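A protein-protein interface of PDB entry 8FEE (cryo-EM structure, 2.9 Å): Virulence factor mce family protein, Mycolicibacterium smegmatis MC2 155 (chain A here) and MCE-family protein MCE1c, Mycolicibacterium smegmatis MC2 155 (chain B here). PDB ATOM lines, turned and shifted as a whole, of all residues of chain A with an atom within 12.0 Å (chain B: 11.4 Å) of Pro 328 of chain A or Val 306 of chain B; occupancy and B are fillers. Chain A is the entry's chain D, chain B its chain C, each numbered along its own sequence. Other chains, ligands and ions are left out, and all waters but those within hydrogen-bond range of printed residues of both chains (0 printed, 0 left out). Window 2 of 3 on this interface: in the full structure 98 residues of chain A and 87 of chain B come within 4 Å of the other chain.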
ATOM      1  N   ILE A 316      33.246   8.203  16.077  1.00  0.00           N
ATOM      2  CA  ILE A 316      32.212   8.535  15.098  1.00  0.00           C
ATOM      3  C   ILE A 316      32.734   8.363  13.674  1.00  0.00           C
ATOM      4  O   ILE A 316      32.005   7.916  12.779  1.00  0.00           O
ATOM      5  CB  ILE A 316      31.690   9.962  15.349  1.00  0.00           C
ATOM      6  CG1 ILE A 316      30.904  10.010  16.656  1.00  0.00           C
ATOM      7  CG2 ILE A 316      30.790  10.415  14.227  1.00  0.00           C
ATOM      8  CD1 ILE A 316      30.280  11.351  16.941  1.00  0.00           C
ATOM      9  N   ILE A 324      32.103  11.933   9.240  1.00  0.00           N
ATOM     10  CA  ILE A 324      31.416  11.550  10.463  1.00  0.00           C
ATOM     11  C   ILE A 324      30.051  10.978  10.101  1.00  0.00           C
ATOM     12  O   ILE A 324      29.643  10.968   8.940  1.00  0.00           O
ATOM     13  CB  ILE A 324      31.280  12.728  11.448  1.00  0.00           C
ATOM     14  CG1 ILE A 324      30.522  13.886  10.803  1.00  0.00           C
ATOM     15  CG2 ILE A 324      32.650  13.184  11.919  1.00  0.00           C
ATOM     16  CD1 ILE A 324      30.673  15.199  11.543  1.00  0.00           C
ATOM     17  N   ILE A 325      29.350  10.481  11.120  1.00  0.00           N
ATOM     18  CA  ILE A 325      28.046   9.846  10.958  1.00  0.00           C
ATOM     19  C   ILE A 325      27.128  10.372  12.051  1.00  0.00           C
ATOM     20  O   ILE A 325      27.533  10.481  13.211  1.00  0.00           O
ATOM     21  CB  ILE A 325      28.142   8.305  11.031  1.00  0.00           C
ATOM     22  CG1 ILE A 325      29.108   7.757   9.980  1.00  0.00           C
ATOM     23  CG2 ILE A 325      26.774   7.666  10.865  1.00  0.00           C
ATOM     24  CD1 ILE A 325      29.316   6.269  10.077  1.00  0.00           C
ATOM     25  N   GLY A 326      25.896  10.690  11.686  1.00  0.00           N
ATOM     26  CA  GLY A 326      24.922  11.155  12.658  1.00  0.00           C
ATOM     27  C   GLY A 326      23.512  10.853  12.210  1.00  0.00           C
ATOM     28  O   GLY A 326      23.202  10.894  11.017  1.00  0.00           O
ATOM     29  N   LEU A 327      22.644  10.561  13.178  1.00  0.00           N
ATOM     30  CA  LEU A 327      21.305  10.156  12.793  1.00  0.00           C
ATOM     31  C   LEU A 327      20.264  11.106  13.371  1.00  0.00           C
ATOM     32  O   LEU A 327      20.414  11.580  14.501  1.00  0.00           O
ATOM     33  CB  LEU A 327      21.004   8.712  13.239  1.00  0.00           C
ATOM     34  CG  LEU A 327      21.051   8.246  14.697  1.00  0.00           C
ATOM     35  CD1 LEU A 327      19.755   8.517  15.453  1.00  0.00           C
ATOM     36  CD2 LEU A 327      21.363   6.764  14.718  1.00  0.00           C
ATOM     37  N   PRO A 328      19.205  11.404  12.621  1.00  0.00           N
ATOM     38  CA  PRO A 328      18.185  12.334  13.111  1.00  0.00           C
ATOM     39  C   PRO A 328      17.349  11.725  14.226  1.00  0.00           C
ATOM     40  O   PRO A 328      17.255  10.506  14.384  1.00  0.00           O
ATOM     41  CB  PRO A 328      17.331  12.611  11.870  1.00  0.00           C
ATOM     42  CG  PRO A 328      17.515  11.403  11.021  1.00  0.00           C
ATOM     43  CD  PRO A 328      18.931  10.959  11.244  1.00  0.00           C
ATOM     44  N   VAL A 329      16.734  12.607  15.007  1.00  0.00           N
ATOM     45  CA  VAL A 329      15.853  12.192  16.091  1.00  0.00           C
ATOM     46  C   VAL A 329      14.399  12.412  15.694  1.00  0.00           C
ATOM     47  O   VAL A 329      13.497  12.322  16.526  1.00  0.00           O
ATOM     48  CB  VAL A 329      16.178  12.941  17.395  1.00  0.00           C
ATOM     49  CG1 VAL A 329      17.603  12.652  17.834  1.00  0.00           C
ATOM     50  CG2 VAL A 329      15.963  14.432  17.216  1.00  0.00           C
ATOM     51  N   ASN A 376       7.012  12.709  24.172  1.00  0.00           N
ATOM     52  CA  ASN A 376       8.422  12.970  23.892  1.00  0.00           C
ATOM     53  C   ASN A 376       8.847  12.362  22.561  1.00  0.00           C
ATOM     54  O   ASN A 376       9.513  13.021  21.754  1.00  0.00           O
ATOM     55  CB  ASN A 376       9.289  12.436  25.032  1.00  0.00           C
ATOM     56  CG  ASN A 376       9.079  13.195  26.327  1.00  0.00           C
ATOM     57  OD1 ASN A 376       8.671  14.355  26.319  1.00  0.00           O
ATOM     58  ND2 ASN A 376       9.360  12.541  27.448  1.00  0.00           N
ATOM     59  N   TYR A 377       8.474  11.110  22.310  1.00  0.00           N
ATOM     60  CA  TYR A 377       8.880  10.421  21.092  1.00  0.00           C
ATOM     61  C   TYR A 377       7.914   9.272  20.832  1.00  0.00           C
ATOM     62  O   TYR A 377       6.972   9.039  21.593  1.00  0.00           O
ATOM     63  CB  TYR A 377      10.325   9.918  21.191  1.00  0.00           C
ATOM     64  CG  TYR A 377      10.638   9.193  22.482  1.00  0.00           C
ATOM     65  CD1 TYR A 377      10.377   7.837  22.622  1.00  0.00           C
ATOM     66  CD2 TYR A 377      11.202   9.863  23.557  1.00  0.00           C
ATOM     67  CE1 TYR A 377      10.659   7.172  23.800  1.00  0.00           C
ATOM     68  CE2 TYR A 377      11.487   9.206  24.736  1.00  0.00           C
ATOM     69  CZ  TYR A 377      11.216   7.861  24.852  1.00  0.00           C
ATOM     70  OH  TYR A 377      11.503   7.204  26.025  1.00  0.00           O
ATOM     71  N   LEU A 378       8.162   8.551  19.740  1.00  0.00           N
ATOM     72  CA  LEU A 378       7.323   7.433  19.334  1.00  0.00           C
ATOM     73  C   LEU A 378       7.610   6.209  20.204  1.00  0.00           C
ATOM     74  O   LEU A 378       8.763   5.964  20.567  1.00  0.00           O
ATOM     75  CB  LEU A 378       7.560   7.092  17.865  1.00  0.00           C
ATOM     76  CG  LEU A 378       7.075   8.133  16.857  1.00  0.00           C
ATOM     77  CD1 LEU A 378       7.504   7.761  15.449  1.00  0.00           C
ATOM     78  CD2 LEU A 378       5.566   8.278  16.940  1.00  0.00           C
ATOM     79  N   PHE A 380       7.797   3.164  19.437  1.00  0.00           N
ATOM     80  CA  PHE A 380       8.495   2.101  18.732  1.00  0.00           C
ATOM     81  C   PHE A 380       9.724   2.648  18.020  1.00  0.00           C
ATOM     82  O   PHE A 380       9.759   3.811  17.608  1.00  0.00           O
ATOM     83  CB  PHE A 380       7.571   1.408  17.721  1.00  0.00           C
ATOM     84  CG  PHE A 380       6.660   2.351  16.987  1.00  0.00           C
ATOM     85  CD1 PHE A 380       7.097   3.014  15.852  1.00  0.00           C
ATOM     86  CD2 PHE A 380       5.365   2.571  17.429  1.00  0.00           C
ATOM     87  CE1 PHE A 380       6.260   3.881  15.175  1.00  0.00           C
ATOM     88  CE2 PHE A 380       4.525   3.437  16.756  1.00  0.00           C
ATOM     89  CZ  PHE A 380       4.973   4.092  15.628  1.00  0.00           C
ATOM     90  N   GLY A 381      10.732   1.790  17.882  1.00  0.00           N
ATOM     91  CA  GLY A 381      11.960   2.163  17.216  1.00  0.00           C
ATOM     92  C   GLY A 381      12.459   1.018  16.361  1.00  0.00           C
ATOM     93  O   GLY A 381      12.091  -0.141  16.562  1.00  0.00           O
ATOM     94  N   MET A 382      13.306   1.359  15.392  1.00  0.00           N
ATOM     95  CA  MET A 382      13.807   0.367  14.456  1.00  0.00           C
ATOM     96  C   MET A 382      15.264   0.660  14.122  1.00  0.00           C
ATOM     97  O   MET A 382      15.731   1.797  14.221  1.00  0.00           O
ATOM     98  CB  MET A 382      12.955   0.336  13.177  1.00  0.00           C
ATOM     99  CG  MET A 382      13.081  -0.943  12.365  1.00  0.00           C
ATOM    100  SD  MET A 382      11.713  -1.169  11.214  1.00  0.00           S
ATOM    101  CE  MET A 382      11.760  -2.945  10.979  1.00  0.00           C
ATOM    102  N   ASN A 383      15.978  -0.394  13.726  1.00  0.00           N
ATOM    103  CA  ASN A 383      17.343  -0.278  13.216  1.00  0.00           C
ATOM    104  C   ASN A 383      17.550  -1.444  12.253  1.00  0.00           C
ATOM    105  O   ASN A 383      17.759  -2.579  12.691  1.00  0.00           O
ATOM    106  CB  ASN A 383      18.364  -0.291  14.345  1.00  0.00           C
ATOM    107  CG  ASN A 383      19.784  -0.104  13.850  1.00  0.00           C
ATOM    108  OD1 ASN A 383      20.516  -1.073  13.647  1.00  0.00           O
ATOM    109  ND2 ASN A 383      20.182   1.146  13.653  1.00  0.00           N
ATOM    110  N   SER B 293      27.522  19.117  28.381  1.00  0.00           N
ATOM    111  CA  SER B 293      26.278  19.093  27.620  1.00  0.00           C
ATOM    112  C   SER B 293      26.532  18.811  26.145  1.00  0.00           C
ATOM    113  O   SER B 293      25.743  18.114  25.497  1.00  0.00           O
ATOM    114  CB  SER B 293      25.531  20.414  27.789  1.00  0.00           C
ATOM    115  OG  SER B 293      24.478  20.516  26.847  1.00  0.00           O
ATOM    116  N   LEU B 294      27.620  19.352  25.593  1.00  0.00           N
ATOM    117  CA  LEU B 294      27.897  19.154  24.174  1.00  0.00           C
ATOM    118  C   LEU B 294      28.352  17.728  23.886  1.00  0.00           C
ATOM    119  O   LEU B 294      27.909  17.119  22.906  1.00  0.00           O
ATOM    120  CB  LEU B 294      28.940  20.163  23.700  1.00  0.00           C
ATOM    121  CG  LEU B 294      29.042  20.359  22.189  1.00  0.00           C
ATOM    122  CD1 LEU B 294      27.802  21.050  21.661  1.00  0.00           C
ATOM    123  CD2 LEU B 294      30.276  21.165  21.846  1.00  0.00           C
ATOM    124  N   GLU B 296      27.458  15.202  25.423  1.00  0.00           N
ATOM    125  CA  GLU B 296      26.371  14.274  25.711  1.00  0.00           C
ATOM    126  C   GLU B 296      25.789  13.665  24.441  1.00  0.00           C
ATOM    127  O   GLU B 296      25.265  12.547  24.475  1.00  0.00           O
ATOM    128  CB  GLU B 296      25.277  14.982  26.511  1.00  0.00           C
ATOM    129  CG  GLU B 296      24.330  14.039  27.229  1.00  0.00           C
ATOM    130  CD  GLU B 296      24.934  13.475  28.502  1.00  0.00           C
ATOM    131  OE1 GLU B 296      26.046  13.903  28.878  1.00  0.00           O
ATOM    132  OE2 GLU B 296      24.306  12.597  29.125  1.00  0.00           O
ATOM    133  N   ALA B 297      25.869  14.383  23.319  1.00  0.00           N
ATOM    134  CA  ALA B 297      25.239  13.923  22.086  1.00  0.00           C
ATOM    135  C   ALA B 297      25.868  12.632  21.582  1.00  0.00           C
ATOM    136  O   ALA B 297      25.163  11.694  21.192  1.00  0.00           O
ATOM    137  CB  ALA B 297      25.321  15.013  21.019  1.00  0.00           C
ATOM    138  N   LEU B 298      27.193  12.560  21.588  1.00  0.00           N
ATOM    139  CA  LEU B 298      27.904  11.396  21.064  1.00  0.00           C
ATOM    140  C   LEU B 298      28.042  10.297  22.115  1.00  0.00           C
ATOM    141  O   LEU B 298      29.135   9.805  22.387  1.00  0.00           O
ATOM    142  CB  LEU B 298      29.271  11.824  20.543  1.00  0.00           C
ATOM    143  CG  LEU B 298      29.689  13.274  20.799  1.00  0.00           C
ATOM    144  CD1 LEU B 298      31.187  13.365  20.866  1.00  0.00           C
ATOM    145  CD2 LEU B 298      29.183  14.202  19.705  1.00  0.00           C
ATOM    146  N   ALA B 299      26.919   9.894  22.710  1.00  0.00           N
ATOM    147  CA  ALA B 299      26.933   8.961  23.827  1.00  0.00           C
ATOM    148  C   ALA B 299      26.092   7.714  23.608  1.00  0.00           C
ATOM    149  O   ALA B 299      26.400   6.678  24.197  1.00  0.00           O
ATOM    150  CB  ALA B 299      26.456   9.651  25.113  1.00  0.00           C
ATOM    151  N   SER B 300      25.031   7.785  22.807  1.00  0.00           N
ATOM    152  CA  SER B 300      24.150   6.636  22.641  1.00  0.00           C
ATOM    153  C   SER B 300      24.703   5.594  21.680  1.00  0.00           C
ATOM    154  O   SER B 300      24.220   4.457  21.679  1.00  0.00           O
ATOM    155  CB  SER B 300      22.771   7.090  22.165  1.00  0.00           C
ATOM    156  OG  SER B 300      22.139   7.900  23.140  1.00  0.00           O
ATOM    157  N   GLY B 301      25.692   5.947  20.864  1.00  0.00           N
ATOM    158  CA  GLY B 301      26.231   5.029  19.891  1.00  0.00           C
ATOM    159  C   GLY B 301      27.496   5.549  19.240  1.00  0.00           C
ATOM    160  O   GLY B 301      28.086   6.541  19.679  1.00  0.00           O
ATOM    161  N   PRO B 302      27.940   4.884  18.168  1.00  0.00           N
ATOM    162  CA  PRO B 302      29.102   5.339  17.394  1.00  0.00           C
ATOM    163  C   PRO B 302      28.772   6.458  16.407  1.00  0.00           C
ATOM    164  O   PRO B 302      29.134   6.401  15.231  1.00  0.00           O
ATOM    165  CB  PRO B 302      29.547   4.062  16.676  1.00  0.00           C
ATOM    166  CG  PRO B 302      28.288   3.306  16.480  1.00  0.00           C
ATOM    167  CD  PRO B 302      27.429   3.591  17.684  1.00  0.00           C
ATOM    168  N   TYR B 303      28.089   7.487  16.897  1.00  0.00           N
ATOM    169  CA  TYR B 303      27.571   8.579  16.081  1.00  0.00           C
ATOM    170  C   TYR B 303      27.150   9.702  17.021  1.00  0.00           C
ATOM    171  O   TYR B 303      27.334   9.617  18.239  1.00  0.00           O
ATOM    172  CB  TYR B 303      26.406   8.107  15.206  1.00  0.00           C
ATOM    173  CG  TYR B 303      25.390   7.273  15.953  1.00  0.00           C
ATOM    174  CD1 TYR B 303      24.435   7.863  16.771  1.00  0.00           C
ATOM    175  CD2 TYR B 303      25.385   5.892  15.835  1.00  0.00           C
ATOM    176  CE1 TYR B 303      23.511   7.101  17.456  1.00  0.00           C
ATOM    177  CE2 TYR B 303      24.462   5.121  16.513  1.00  0.00           C
ATOM    178  CZ  TYR B 303      23.528   5.729  17.321  1.00  0.00           C
ATOM    179  OH  TYR B 303      22.611   4.958  17.994  1.00  0.00           O
ATOM    180  N   PHE B 304      26.580  10.758  16.445  1.00  0.00           N
ATOM    181  CA  PHE B 304      26.032  11.867  17.211  1.00  0.00           C
ATOM    182  C   PHE B 304      24.608  12.152  16.762  1.00  0.00           C
ATOM    183  O   PHE B 304      24.303  12.094  15.571  1.00  0.00           O
ATOM    184  CB  PHE B 304      26.901  13.130  17.073  1.00  0.00           C
ATOM    185  CG  PHE B 304      27.072  13.614  15.657  1.00  0.00           C
ATOM    186  CD1 PHE B 304      26.232  14.579  15.125  1.00  0.00           C
ATOM    187  CD2 PHE B 304      28.096  13.125  14.868  1.00  0.00           C
ATOM    188  CE1 PHE B 304      26.406  15.026  13.830  1.00  0.00           C
ATOM    189  CE2 PHE B 304      28.268  13.568  13.574  1.00  0.00           C
ATOM    190  CZ  PHE B 304      27.423  14.521  13.055  1.00  0.00           C
ATOM    191  N   LYS B 305      23.737  12.455  17.718  1.00  0.00           N
ATOM    192  CA  LYS B 305      22.371  12.815  17.372  1.00  0.00           C
ATOM    193  C   LYS B 305      22.314  14.216  16.776  1.00  0.00           C
ATOM    194  O   LYS B 305      23.135  15.083  17.083  1.00  0.00           O
ATOM    195  CB  LYS B 305      21.461  12.742  18.595  1.00  0.00           C
ATOM    196  CG  LYS B 305      21.333  11.360  19.192  1.00  0.00           C
ATOM    197  CD  LYS B 305      20.200  11.313  20.195  1.00  0.00           C
ATOM    198  CE  LYS B 305      20.351  10.119  21.108  1.00  0.00           C
ATOM    199  NZ  LYS B 305      20.793   8.937  20.327  1.00  0.00           N
ATOM    200  N   VAL B 306      21.323  14.427  15.912  1.00  0.00           N
ATOM    201  CA  VAL B 306      21.027  15.735  15.344  1.00  0.00           C
ATOM    202  C   VAL B 306      19.519  15.917  15.307  1.00  0.00           C
ATOM    203  O   VAL B 306      18.762  14.956  15.146  1.00  0.00           O
ATOM    204  CB  VAL B 306      21.619  15.914  13.930  1.00  0.00           C
ATOM    205  CG1 VAL B 306      23.119  16.055  13.993  1.00  0.00           C
ATOM    206  CG2 VAL B 306      21.242  14.739  13.045  1.00  0.00           C
ATOM    207  N   MET B 307      19.084  17.159  15.475  1.00  0.00           N
ATOM    208  CA  MET B 307      17.683  17.528  15.329  1.00  0.00           C
ATOM    209  C   MET B 307      17.547  18.389  14.081  1.00  0.00           C
ATOM    210  O   MET B 307      18.199  19.432  13.971  1.00  0.00           O
ATOM    211  CB  MET B 307      17.164  18.272  16.557  1.00  0.00           C
ATOM    212  CG  MET B 307      15.669  18.526  16.508  1.00  0.00           C
ATOM    213  SD  MET B 307      15.030  19.421  17.933  1.00  0.00           S
ATOM    214  CE  MET B 307      13.276  19.383  17.579  1.00  0.00           C
ATOM    215  N   LEU B 308      16.709  17.952  13.150  1.00  0.00           N
ATOM    216  CA  LEU B 308      16.468  18.672  11.903  1.00  0.00           C
ATOM    217  C   LEU B 308      15.067  19.268  11.978  1.00  0.00           C
ATOM    218  O   LEU B 308      14.069  18.556  11.837  1.00  0.00           O
ATOM    219  CB  LEU B 308      16.625  17.742  10.704  1.00  0.00           C
ATOM    220  CG  LEU B 308      17.990  17.068  10.557  1.00  0.00           C
ATOM    221  CD1 LEU B 308      17.911  15.894   9.597  1.00  0.00           C
ATOM    222  CD2 LEU B 308      19.024  18.072  10.086  1.00  0.00           C
ATOM    223  N   VAL B 309      14.999  20.584  12.208  1.00  0.00           N
ATOM    224  CA  VAL B 309      13.717  21.277  12.324  1.00  0.00           C
ATOM    225  C   VAL B 309      13.122  21.591  10.959  1.00  0.00           C
ATOM    226  O   VAL B 309      11.966  22.024  10.869  1.00  0.00           O
ATOM    227  CB  VAL B 309      13.980  22.508  13.224  1.00  0.00           C
ATOM    228  CG1 VAL B 309      12.762  23.423  13.372  1.00  0.00           C
ATOM    229  CG2 VAL B 309      14.479  22.064  14.590  1.00  0.00           C
ATOM    230  N   ASN B 310      13.841  21.294   9.882  1.00  0.00           N
ATOM    231  CA  ASN B 310      13.309  21.463   8.537  1.00  0.00           C
ATOM    232  C   ASN B 310      12.859  20.128   7.953  1.00  0.00           C
ATOM    233  O   ASN B 310      13.677  19.330   7.495  1.00  0.00           O
ATOM    234  CB  ASN B 310      14.354  22.109   7.630  1.00  0.00           C
ATOM    235  CG  ASN B 310      14.750  23.492   8.096  1.00  0.00           C
ATOM    236  OD1 ASN B 310      15.870  23.707   8.554  1.00  0.00           O
ATOM    237  ND2 ASN B 310      13.830  24.441   7.979  1.00  0.00           N
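The backbone carbonyl oxygen of Ile 325 of chain A sits close to the backbone NH of Phe 304 of chain B (3.4 Å). N of Leu 327 of chain A lies within hydrogen-bond range of O of Phe 304 of chain B (3.3 Å). The backbone NH (N) of Val 306 of chain B is in hydrogen-bond range of the backbone carbonyl oxygen (O) of Leu 327 of chain A, 3.3 Å away. The backbone carbonyl oxygen of Val 306 of chain B is in hydrogen-bond range of the backbone NH of Val 329 of chain A (3.1 Å).
The side-chain hydroxyl (OG) of Ser 300 of chain B sits close to the side-chain amino group (NZ) of Lys 305 of chain B, at 3.3 Å.
Among the printed residues, merely in contact across the chains: Ile 316 of chain A with Leu 298 of chain B (3.8 Å), Ile 316 of chain A with Pro 302 of chain B (3.7 Å), Ile 316 of chain A with Tyr 303 of chain B (3.5 Å), Ile 316 of chain A with Phe 304 of chain B (3.5 Å), Ile 324 of chain A with Phe 304 of chain B (3.5 Å), Ile 325 of chain A with Tyr 303 of chain B (3.3 Å), Gly 326 of chain A with Phe 304 of chain B (3.1 Å), Leu 327 of chain A with Tyr 303 of chain B (3.5 Å), Leu 327 of chain A with Lys 305 of chain B (3.7 Å), Pro 328 of chain A with Val 306 of chain B (3.4 Å) and Val 329 of chain A with Lys 305 of chain B (3.8 Å).
Of chain B, only Val 306 (3.4 Å) comes within 4 Å of Pro 328 of chain A. Of chain A, only Leu 327, Pro 328 and Val 329 come within 4 Å of Val 306 of chain B. Gly 326 of chain A touches one residue of chain B. Of the printed residues of chain B, Leu 327 of chain A touches Tyr 303 (3.5 Å), Phe 304 (3.3 Å), Lys 305 (3.7 Å) and Val 306 (3.3 Å). Phe 304 of chain B touches just these residues of chain A: Ile 316, Ile 324, Ile 325, Gly 326 and Leu 327. Printed residues of chain B within 4 Å of Val 329 of chain A: Lys 305 (3.8 Å) and Val 306 (3.1 Å). Of the printed residues of chain A, Leu 298 of chain B touches Ile 316 (3.8 Å). Printed residues of chain A within 4 Å of Pro 302 of chain B: Ile 316 (3.7 Å). Of the printed residues of chain A, Tyr 303 of chain B touches Ile 316, Ile 325 and Leu 327. Asn 376 of chain A touches none of the printed residues of chain B. The nearest residue of chain B that does not touch Pro 328 of chain A is Leu 308 of chain B (4.03 Å). The nearest residue of chain A that does not touch Val 306 of chain B is Gly 326 of chain A (4.6 Å). The nearest printed residue of chain A that does not touch Tyr 303 of chain B is Gly 326 of chain A (4.2 Å).
Along chain A the printed residues that touch a printed residue of chain B span positions 316 to 329. Printed residues of chain B that touch a printed residue of chain A: Leu 298, Pro 302, Tyr 303, Phe 304, Lys 305 and Val 306. Hydrophobic or aromatic side chains of chain B that line the printed part of chain A: Leu 298, Tyr 303, Phe 304 and Val 306. Among the printed residues, 15 pairs touch across the chains.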
